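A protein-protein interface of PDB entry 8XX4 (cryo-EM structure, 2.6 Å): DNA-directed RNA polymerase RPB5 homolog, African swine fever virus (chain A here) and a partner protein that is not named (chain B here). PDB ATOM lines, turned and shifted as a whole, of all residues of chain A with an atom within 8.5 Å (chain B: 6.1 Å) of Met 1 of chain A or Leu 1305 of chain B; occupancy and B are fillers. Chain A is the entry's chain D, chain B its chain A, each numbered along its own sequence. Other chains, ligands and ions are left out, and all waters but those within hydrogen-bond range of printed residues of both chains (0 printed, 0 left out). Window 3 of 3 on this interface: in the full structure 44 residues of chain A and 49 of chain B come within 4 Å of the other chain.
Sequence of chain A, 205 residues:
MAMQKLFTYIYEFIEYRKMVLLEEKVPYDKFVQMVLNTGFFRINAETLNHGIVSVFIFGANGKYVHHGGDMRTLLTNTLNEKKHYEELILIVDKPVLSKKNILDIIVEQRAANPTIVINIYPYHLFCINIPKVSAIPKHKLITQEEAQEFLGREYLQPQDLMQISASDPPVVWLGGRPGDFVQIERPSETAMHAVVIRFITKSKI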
ATOM      1  N   MET A   1      13.457  23.165  29.821  1.00  0.00           N
ATOM      2  CA  MET A   1      13.050  23.952  28.663  1.00  0.00           C
ATOM      3  C   MET A   1      14.137  24.949  28.290  1.00  0.00           C
ATOM      4  O   MET A   1      15.046  25.205  29.077  1.00  0.00           O
ATOM      5  CB  MET A   1      11.732  24.678  28.938  1.00  0.00           C
ATOM      6  CG  MET A   1      10.745  23.880  29.781  1.00  0.00           C
ATOM      7  SD  MET A   1       9.764  22.716  28.811  1.00  0.00           S
ATOM      8  CE  MET A   1       8.397  23.755  28.303  1.00  0.00           C
ATOM      9  N   ALA A   2      14.038  25.505  27.081  1.00  0.00           N
ATOM     10  CA  ALA A   2      15.060  26.432  26.605  1.00  0.00           C
ATOM     11  C   ALA A   2      15.115  27.689  27.460  1.00  0.00           C
ATOM     12  O   ALA A   2      16.200  28.204  27.744  1.00  0.00           O
ATOM     13  CB  ALA A   2      14.804  26.795  25.145  1.00  0.00           C
ATOM     14  N   MET A   3      13.956  28.204  27.870  1.00  0.00           N
ATOM     15  CA  MET A   3      13.931  29.431  28.659  1.00  0.00           C
ATOM     16  C   MET A   3      14.555  29.225  30.034  1.00  0.00           C
ATOM     17  O   MET A   3      15.318  30.072  30.508  1.00  0.00           O
ATOM     18  CB  MET A   3      12.497  29.935  28.788  1.00  0.00           C
ATOM     19  CG  MET A   3      12.097  30.953  27.738  1.00  0.00           C
ATOM     20  SD  MET A   3      13.310  32.267  27.522  1.00  0.00           S
ATOM     21  CE  MET A   3      13.736  32.043  25.799  1.00  0.00           C
ATOM     22  N   GLN A   4      14.245  28.105  30.690  1.00  0.00           N
ATOM     23  CA  GLN A   4      14.796  27.847  32.018  1.00  0.00           C
ATOM     24  C   GLN A   4      16.307  27.652  31.964  1.00  0.00           C
ATOM     25  O   GLN A   4      17.046  28.202  32.790  1.00  0.00           O
ATOM     26  CB  GLN A   4      14.112  26.626  32.636  1.00  0.00           C
ATOM     27  CG  GLN A   4      14.806  26.063  33.869  1.00  0.00           C
ATOM     28  CD  GLN A   4      14.717  26.988  35.069  1.00  0.00           C
ATOM     29  OE1 GLN A   4      13.739  26.963  35.813  1.00  0.00           O
ATOM     30  NE2 GLN A   4      15.746  27.805  35.266  1.00  0.00           N
ATOM     31  N   LYS A   5      16.783  26.866  30.994  1.00  0.00           N
ATOM     32  CA  LYS A   5      18.219  26.664  30.838  1.00  0.00           C
ATOM     33  C   LYS A   5      18.922  27.967  30.486  1.00  0.00           C
ATOM     34  O   LYS A   5      20.008  28.256  31.002  1.00  0.00           O
ATOM     35  CB  LYS A   5      18.487  25.604  29.774  1.00  0.00           C
ATOM     36  CG  LYS A   5      18.041  24.211  30.165  1.00  0.00           C
ATOM     37  CD  LYS A   5      18.741  23.754  31.430  1.00  0.00           C
ATOM     38  CE  LYS A   5      18.362  22.334  31.788  1.00  0.00           C
ATOM     39  NZ  LYS A   5      16.906  22.101  31.601  1.00  0.00           N
ATOM     40  N   LEU A   6      18.316  28.766  29.607  1.00  0.00           N
ATOM     41  CA  LEU A   6      18.873  30.072  29.281  1.00  0.00           C
ATOM     42  C   LEU A   6      18.989  30.934  30.525  1.00  0.00           C
ATOM     43  O   LEU A   6      20.014  31.583  30.752  1.00  0.00           O
ATOM     44  CB  LEU A   6      18.001  30.764  28.240  1.00  0.00           C
ATOM     45  CG  LEU A   6      18.512  30.901  26.814  1.00  0.00           C
ATOM     46  CD1 LEU A   6      17.367  31.343  25.943  1.00  0.00           C
ATOM     47  CD2 LEU A   6      19.642  31.900  26.746  1.00  0.00           C
ATOM     48  N   PHE A   7      17.943  30.946  31.353  1.00  0.00           N
ATOM     49  CA  PHE A   7      17.958  31.774  32.549  1.00  0.00           C
ATOM     50  C   PHE A   7      19.032  31.319  33.527  1.00  0.00           C
ATOM     51  O   PHE A   7      19.703  32.149  34.149  1.00  0.00           O
ATOM     52  CB  PHE A   7      16.589  31.756  33.220  1.00  0.00           C
ATOM     53  CG  PHE A   7      16.480  32.697  34.376  1.00  0.00           C
ATOM     54  CD1 PHE A   7      16.562  34.063  34.180  1.00  0.00           C
ATOM     55  CD2 PHE A   7      16.313  32.218  35.661  1.00  0.00           C
ATOM     56  CE1 PHE A   7      16.469  34.930  35.239  1.00  0.00           C
ATOM     57  CE2 PHE A   7      16.220  33.083  36.724  1.00  0.00           C
ATOM     58  CZ  PHE A   7      16.298  34.440  36.512  1.00  0.00           C
ATOM     59  N   THR A   8      19.205  30.009  33.688  1.00  0.00           N
ATOM     60  CA  THR A   8      20.195  29.549  34.653  1.00  0.00           C
ATOM     61  C   THR A   8      21.625  29.638  34.138  1.00  0.00           C
ATOM     62  O   THR A   8      22.550  29.702  34.954  1.00  0.00           O
ATOM     63  CB  THR A   8      19.915  28.112  35.097  1.00  0.00           C
ATOM     64  OG1 THR A   8      20.938  27.698  36.010  1.00  0.00           O
ATOM     65  CG2 THR A   8      19.923  27.175  33.923  1.00  0.00           C
ATOM     66  N   TYR A   9      21.841  29.655  32.820  1.00  0.00           N
ATOM     67  CA  TYR A   9      23.196  29.620  32.291  1.00  0.00           C
ATOM     68  C   TYR A   9      23.667  30.928  31.675  1.00  0.00           C
ATOM     69  O   TYR A   9      24.862  31.058  31.394  1.00  0.00           O
ATOM     70  CB  TYR A   9      23.332  28.498  31.255  1.00  0.00           C
ATOM     71  CG  TYR A   9      23.356  27.129  31.878  1.00  0.00           C
ATOM     72  CD1 TYR A   9      24.294  26.806  32.845  1.00  0.00           C
ATOM     73  CD2 TYR A   9      22.432  26.164  31.514  1.00  0.00           C
ATOM     74  CE1 TYR A   9      24.314  25.562  33.426  1.00  0.00           C
ATOM     75  CE2 TYR A   9      22.446  24.916  32.089  1.00  0.00           C
ATOM     76  CZ  TYR A   9      23.387  24.620  33.044  1.00  0.00           C
ATOM     77  OH  TYR A   9      23.405  23.374  33.618  1.00  0.00           O
ATOM     78  N   TYR A  28      12.873  33.589  38.272  1.00  0.00           N
ATOM     79  CA  TYR A  28      12.633  32.990  36.963  1.00  0.00           C
ATOM     80  C   TYR A  28      11.242  33.323  36.444  1.00  0.00           C
ATOM     81  O   TYR A  28      11.063  33.571  35.247  1.00  0.00           O
ATOM     82  CB  TYR A  28      12.823  31.476  37.028  1.00  0.00           C
ATOM     83  CG  TYR A  28      12.292  30.758  35.809  1.00  0.00           C
ATOM     84  CD1 TYR A  28      12.825  31.003  34.552  1.00  0.00           C
ATOM     85  CD2 TYR A  28      11.254  29.845  35.912  1.00  0.00           C
ATOM     86  CE1 TYR A  28      12.342  30.357  33.435  1.00  0.00           C
ATOM     87  CE2 TYR A  28      10.765  29.192  34.800  1.00  0.00           C
ATOM     88  CZ  TYR A  28      11.313  29.454  33.563  1.00  0.00           C
ATOM     89  OH  TYR A  28      10.831  28.807  32.452  1.00  0.00           O
ATOM     90  N   ASP A  93      15.796  32.530  18.935  1.00  0.00           N
ATOM     91  CA  ASP A  93      15.589  31.146  18.559  1.00  0.00           C
ATOM     92  C   ASP A  93      16.358  30.842  17.280  1.00  0.00           C
ATOM     93  O   ASP A  93      16.646  31.728  16.474  1.00  0.00           O
ATOM     94  CB  ASP A  93      14.101  30.863  18.367  1.00  0.00           C
ATOM     95  CG  ASP A  93      13.740  29.429  18.672  1.00  0.00           C
ATOM     96  OD1 ASP A  93      14.621  28.682  19.146  1.00  0.00           O
ATOM     97  OD2 ASP A  93      12.577  29.046  18.436  1.00  0.00           O
ATOM     98  N   TYR A 123      19.631  30.024  20.816  1.00  0.00           N
ATOM     99  CA  TYR A 123      19.365  29.675  22.208  1.00  0.00           C
ATOM    100  C   TYR A 123      20.382  28.677  22.743  1.00  0.00           C
ATOM    101  O   TYR A 123      20.860  28.818  23.873  1.00  0.00           O
ATOM    102  CB  TYR A 123      17.958  29.104  22.345  1.00  0.00           C
ATOM    103  CG  TYR A 123      16.864  30.136  22.364  1.00  0.00           C
ATOM    104  CD1 TYR A 123      17.151  31.478  22.542  1.00  0.00           C
ATOM    105  CD2 TYR A 123      15.539  29.765  22.205  1.00  0.00           C
ATOM    106  CE1 TYR A 123      16.150  32.420  22.564  1.00  0.00           C
ATOM    107  CE2 TYR A 123      14.533  30.698  22.220  1.00  0.00           C
ATOM    108  CZ  TYR A 123      14.843  32.023  22.402  1.00  0.00           C
ATOM    109  OH  TYR A 123      13.838  32.957  22.420  1.00  0.00           O
ATOM    110  N   HIS A 124      20.727  27.663  21.947  1.00  0.00           N
ATOM    111  CA  HIS A 124      21.539  26.559  22.444  1.00  0.00           C
ATOM    112  C   HIS A 124      22.946  26.983  22.831  1.00  0.00           C
ATOM    113  O   HIS A 124      23.644  26.212  23.494  1.00  0.00           O
ATOM    114  CB  HIS A 124      21.604  25.437  21.406  1.00  0.00           C
ATOM    115  CG  HIS A 124      22.182  25.848  20.088  1.00  0.00           C
ATOM    116  ND1 HIS A 124      23.518  26.133  19.914  1.00  0.00           N
ATOM    117  CD2 HIS A 124      21.605  25.996  18.872  1.00  0.00           C
ATOM    118  CE1 HIS A 124      23.738  26.451  18.653  1.00  0.00           C
ATOM    119  NE2 HIS A 124      22.594  26.376  17.998  1.00  0.00           N
ATOM    120  N   PHE A 126      23.740  29.272  24.914  1.00  0.00           N
ATOM    121  CA  PHE A 126      23.740  29.637  26.325  1.00  0.00           C
ATOM    122  C   PHE A 126      22.792  28.769  27.140  1.00  0.00           C
ATOM    123  O   PHE A 126      22.426  29.138  28.257  1.00  0.00           O
ATOM    124  CB  PHE A 126      23.378  31.112  26.497  1.00  0.00           C
ATOM    125  CG  PHE A 126      24.133  32.025  25.588  1.00  0.00           C
ATOM    126  CD1 PHE A 126      25.347  32.553  25.973  1.00  0.00           C
ATOM    127  CD2 PHE A 126      23.634  32.352  24.346  1.00  0.00           C
ATOM    128  CE1 PHE A 126      26.045  33.389  25.139  1.00  0.00           C
ATOM    129  CE2 PHE A 126      24.330  33.188  23.508  1.00  0.00           C
ATOM    130  CZ  PHE A 126      25.535  33.708  23.906  1.00  0.00           C
ATOM    131  N   CYS A 127      22.384  27.627  26.600  1.00  0.00           N
ATOM    132  CA  CYS A 127      21.524  26.691  27.306  1.00  0.00           C
ATOM    133  C   CYS A 127      22.312  25.655  28.090  1.00  0.00           C
ATOM    134  O   CYS A 127      21.714  24.728  28.644  1.00  0.00           O
ATOM    135  CB  CYS A 127      20.585  25.992  26.323  1.00  0.00           C
ATOM    136  SG  CYS A 127      19.144  26.965  25.867  1.00  0.00           S
ATOM    137  N   ILE A 128      23.637  25.787  28.139  1.00  0.00           N
ATOM    138  CA  ILE A 128      24.494  24.853  28.856  1.00  0.00           C
ATOM    139  C   ILE A 128      25.797  25.573  29.145  1.00  0.00           C
ATOM    140  O   ILE A 128      26.159  26.525  28.450  1.00  0.00           O
ATOM    141  CB  ILE A 128      24.718  23.559  28.035  1.00  0.00           C
ATOM    142  CG1 ILE A 128      25.274  22.445  28.916  1.00  0.00           C
ATOM    143  CG2 ILE A 128      25.636  23.821  26.862  1.00  0.00           C
ATOM    144  CD1 ILE A 128      25.407  21.137  28.201  1.00  0.00           C
ATOM    145  N   ILE B1262      11.404  14.357  23.091  1.00  0.00           N
ATOM    146  CA  ILE B1262      12.127  15.422  22.400  1.00  0.00           C
ATOM    147  C   ILE B1262      12.200  15.097  20.913  1.00  0.00           C
ATOM    148  O   ILE B1262      12.316  13.921  20.540  1.00  0.00           O
ATOM    149  CB  ILE B1262      13.520  15.631  23.016  1.00  0.00           C
ATOM    150  CG1 ILE B1262      14.223  14.293  23.219  1.00  0.00           C
ATOM    151  CG2 ILE B1262      13.412  16.376  24.336  1.00  0.00           C
ATOM    152  CD1 ILE B1262      15.455  14.380  24.079  1.00  0.00           C
ATOM    153  N   ILE B1300      20.957  16.777  20.207  1.00  0.00           N
ATOM    154  CA  ILE B1300      21.817  17.235  21.296  1.00  0.00           C
ATOM    155  C   ILE B1300      21.181  18.379  22.071  1.00  0.00           C
ATOM    156  O   ILE B1300      21.167  18.365  23.303  1.00  0.00           O
ATOM    157  CB  ILE B1300      23.200  17.670  20.780  1.00  0.00           C
ATOM    158  CG1 ILE B1300      23.953  16.499  20.158  1.00  0.00           C
ATOM    159  CG2 ILE B1300      24.020  18.254  21.910  1.00  0.00           C
ATOM    160  CD1 ILE B1300      25.339  16.869  19.703  1.00  0.00           C
ATOM    161  N   PHE B1301      20.644  19.372  21.361  1.00  0.00           N
ATOM    162  CA  PHE B1301      20.001  20.492  22.039  1.00  0.00           C
ATOM    163  C   PHE B1301      18.814  20.024  22.870  1.00  0.00           C
ATOM    164  O   PHE B1301      18.650  20.443  24.024  1.00  0.00           O
ATOM    165  CB  PHE B1301      19.564  21.537  21.014  1.00  0.00           C
ATOM    166  CG  PHE B1301      18.964  22.773  21.620  1.00  0.00           C
ATOM    167  CD1 PHE B1301      19.401  23.245  22.843  1.00  0.00           C
ATOM    168  CD2 PHE B1301      17.972  23.470  20.957  1.00  0.00           C
ATOM    169  CE1 PHE B1301      18.855  24.381  23.394  1.00  0.00           C
ATOM    170  CE2 PHE B1301      17.427  24.606  21.505  1.00  0.00           C
ATOM    171  CZ  PHE B1301      17.870  25.063  22.724  1.00  0.00           C
ATOM    172  N   GLY B1302      17.983  19.146  22.309  1.00  0.00           N
ATOM    173  CA  GLY B1302      16.859  18.617  23.058  1.00  0.00           C
ATOM    174  C   GLY B1302      17.277  17.821  24.275  1.00  0.00           C
ATOM    175  O   GLY B1302      16.587  17.835  25.296  1.00  0.00           O
ATOM    176  N   ALA B1303      18.400  17.109  24.185  1.00  0.00           N
ATOM    177  CA  ALA B1303      18.883  16.343  25.327  1.00  0.00           C
ATOM    178  C   ALA B1303      19.473  17.251  26.401  1.00  0.00           C
ATOM    179  O   ALA B1303      19.346  16.965  27.596  1.00  0.00           O
ATOM    180  CB  ALA B1303      19.906  15.309  24.867  1.00  0.00           C
ATOM    181  N   MET B1304      20.133  18.342  26.000  1.00  0.00           N
ATOM    182  CA  MET B1304      20.586  19.319  26.986  1.00  0.00           C
ATOM    183  C   MET B1304      19.405  19.976  27.680  1.00  0.00           C
ATOM    184  O   MET B1304      19.468  20.275  28.877  1.00  0.00           O
ATOM    185  CB  MET B1304      21.472  20.386  26.340  1.00  0.00           C
ATOM    186  CG  MET B1304      22.620  19.855  25.512  1.00  0.00           C
ATOM    187  SD  MET B1304      23.547  21.151  24.669  1.00  0.00           S
ATOM    188  CE  MET B1304      22.395  22.516  24.741  1.00  0.00           C
ATOM    189  N   LEU B1305      18.322  20.222  26.942  1.00  0.00           N
ATOM    190  CA  LEU B1305      17.129  20.784  27.562  1.00  0.00           C
ATOM    191  C   LEU B1305      16.507  19.819  28.564  1.00  0.00           C
ATOM    192  O   LEU B1305      15.924  20.257  29.561  1.00  0.00           O
ATOM    193  CB  LEU B1305      16.112  21.168  26.492  1.00  0.00           C
ATOM    194  CG  LEU B1305      16.512  22.347  25.609  1.00  0.00           C
ATOM    195  CD1 LEU B1305      15.309  22.902  24.879  1.00  0.00           C
ATOM    196  CD2 LEU B1305      17.180  23.421  26.440  1.00  0.00           C
ATOM    197  N   ASP B1306      16.614  18.516  28.319  1.00  0.00           N
ATOM    198  CA  ASP B1306      16.059  17.531  29.237  1.00  0.00           C
ATOM    199  C   ASP B1306      16.840  17.525  30.544  1.00  0.00           C
ATOM    200  O   ASP B1306      18.074  17.565  30.544  1.00  0.00           O
ATOM    201  CB  ASP B1306      16.080  16.144  28.602  1.00  0.00           C
ATOM    202  CG  ASP B1306      15.252  15.142  29.372  1.00  0.00           C
ATOM    203  OD1 ASP B1306      15.772  14.563  30.346  1.00  0.00           O
ATOM    204  OD2 ASP B1306      14.076  14.936  29.010  1.00  0.00           O
ATOM    205  N   ASP B1307      16.120  17.465  31.659  1.00  0.00           N
ATOM    206  CA  ASP B1307      16.723  17.551  32.980  1.00  0.00           C
ATOM    207  C   ASP B1307      17.008  16.192  33.603  1.00  0.00           C
ATOM    208  O   ASP B1307      17.549  16.137  34.711  1.00  0.00           O
ATOM    209  CB  ASP B1307      15.820  18.361  33.912  1.00  0.00           C
ATOM    210  CG  ASP B1307      16.596  19.080  34.994  1.00  0.00           C
ATOM    211  OD1 ASP B1307      17.721  19.541  34.713  1.00  0.00           O
ATOM    212  OD2 ASP B1307      16.080  19.183  36.126  1.00  0.00           O
ATOM    213  N   PRO B1311      23.827  16.647  30.810  1.00  0.00           N
ATOM    214  CA  PRO B1311      24.010  17.418  29.577  1.00  0.00           C
ATOM    215  C   PRO B1311      25.459  17.592  29.170  1.00  0.00           C
ATOM    216  O   PRO B1311      25.717  17.934  28.009  1.00  0.00           O
ATOM    217  CB  PRO B1311      23.365  18.765  29.915  1.00  0.00           C
ATOM    218  CG  PRO B1311      23.562  18.899  31.384  1.00  0.00           C
ATOM    219  CD  PRO B1311      23.533  17.512  31.966  1.00  0.00           C
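Printed residues of chain A that touch a printed residue of chain B: Met 1, Ala 2, Lys 5, His 124, Cys 127 and Ile 128. Among the printed residues, 8 pairs touch across the chains.
NZ of Lys 5 of chain A lies within hydrogen-bond range of O of Leu 1305 of chain B (2.9 Å).
SG of Cys 127 of chain A is in hydrogen-bond range of O of Ala 2 of chain A (3.7 Å). The backbone carbonyl oxygen of Tyr 123 of chain A lies within hydrogen-bond range of the side-chain sulfur of Cys 127 of chain A (3.2 Å).
Among the printed residues, pairs that only touch across the chains: Met 1 of chain A with Leu 1305 of chain B (3.8 Å), Ala 2 of chain A with Leu 1305 of chain B (3.6 Å), Lys 5 of chain A with Met 1304 of chain B (3.7 Å), His 124 of chain A with Phe 1301 of chain B (3.4 Å), Cys 127 of chain A with Phe 1301 of chain B (3.6 Å), Ile 128 of chain A with Met 1304 of chain B (3.99 Å) and Ile 128 of chain A with Pro 1311 of chain B (3.2 Å).
Met 1 of chain A touches one residue of chain B. Of the printed residues of chain B, Ala 2 of chain A touches Leu 1305 (3.6 Å). Printed residues of chain B within 4 Å of Lys 5 of chain A: Met 1304 (3.7 Å) and Leu 1305 (2.9 Å). Tyr 123 of chain A touches none of the printed residues of chain B. Printed residues of chain B within 4 Å of His 124 of chain A: Phe 1301. Of the printed residues of chain B, Ile 128 of chain A touches Met 1304 (3.99 Å) and Pro 1311 (3.2 Å). Printed residues of chain A within 4 Å of Met 1304 of chain B: Lys 5 and Ile 128. Leu 1305 of chain B touches just these residues of chain A: Met 1 (3.8 Å), Ala 2 (3.6 Å) and Lys 5 (2.9 Å). Asp 1306 of chain B touches none of the printed residues of chain A. The nearest residue of chain B that does not touch Met 1 of chain A is Asp 1306 of chain B (5.8 Å). The nearest residue of chain A that does not touch Leu 1305 of chain B is Cys 127 of chain A (4.1 Å). The nearest printed residue of chain A that does not touch Pro 1311 of chain B is Tyr 9 of chain A (5.0 Å).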
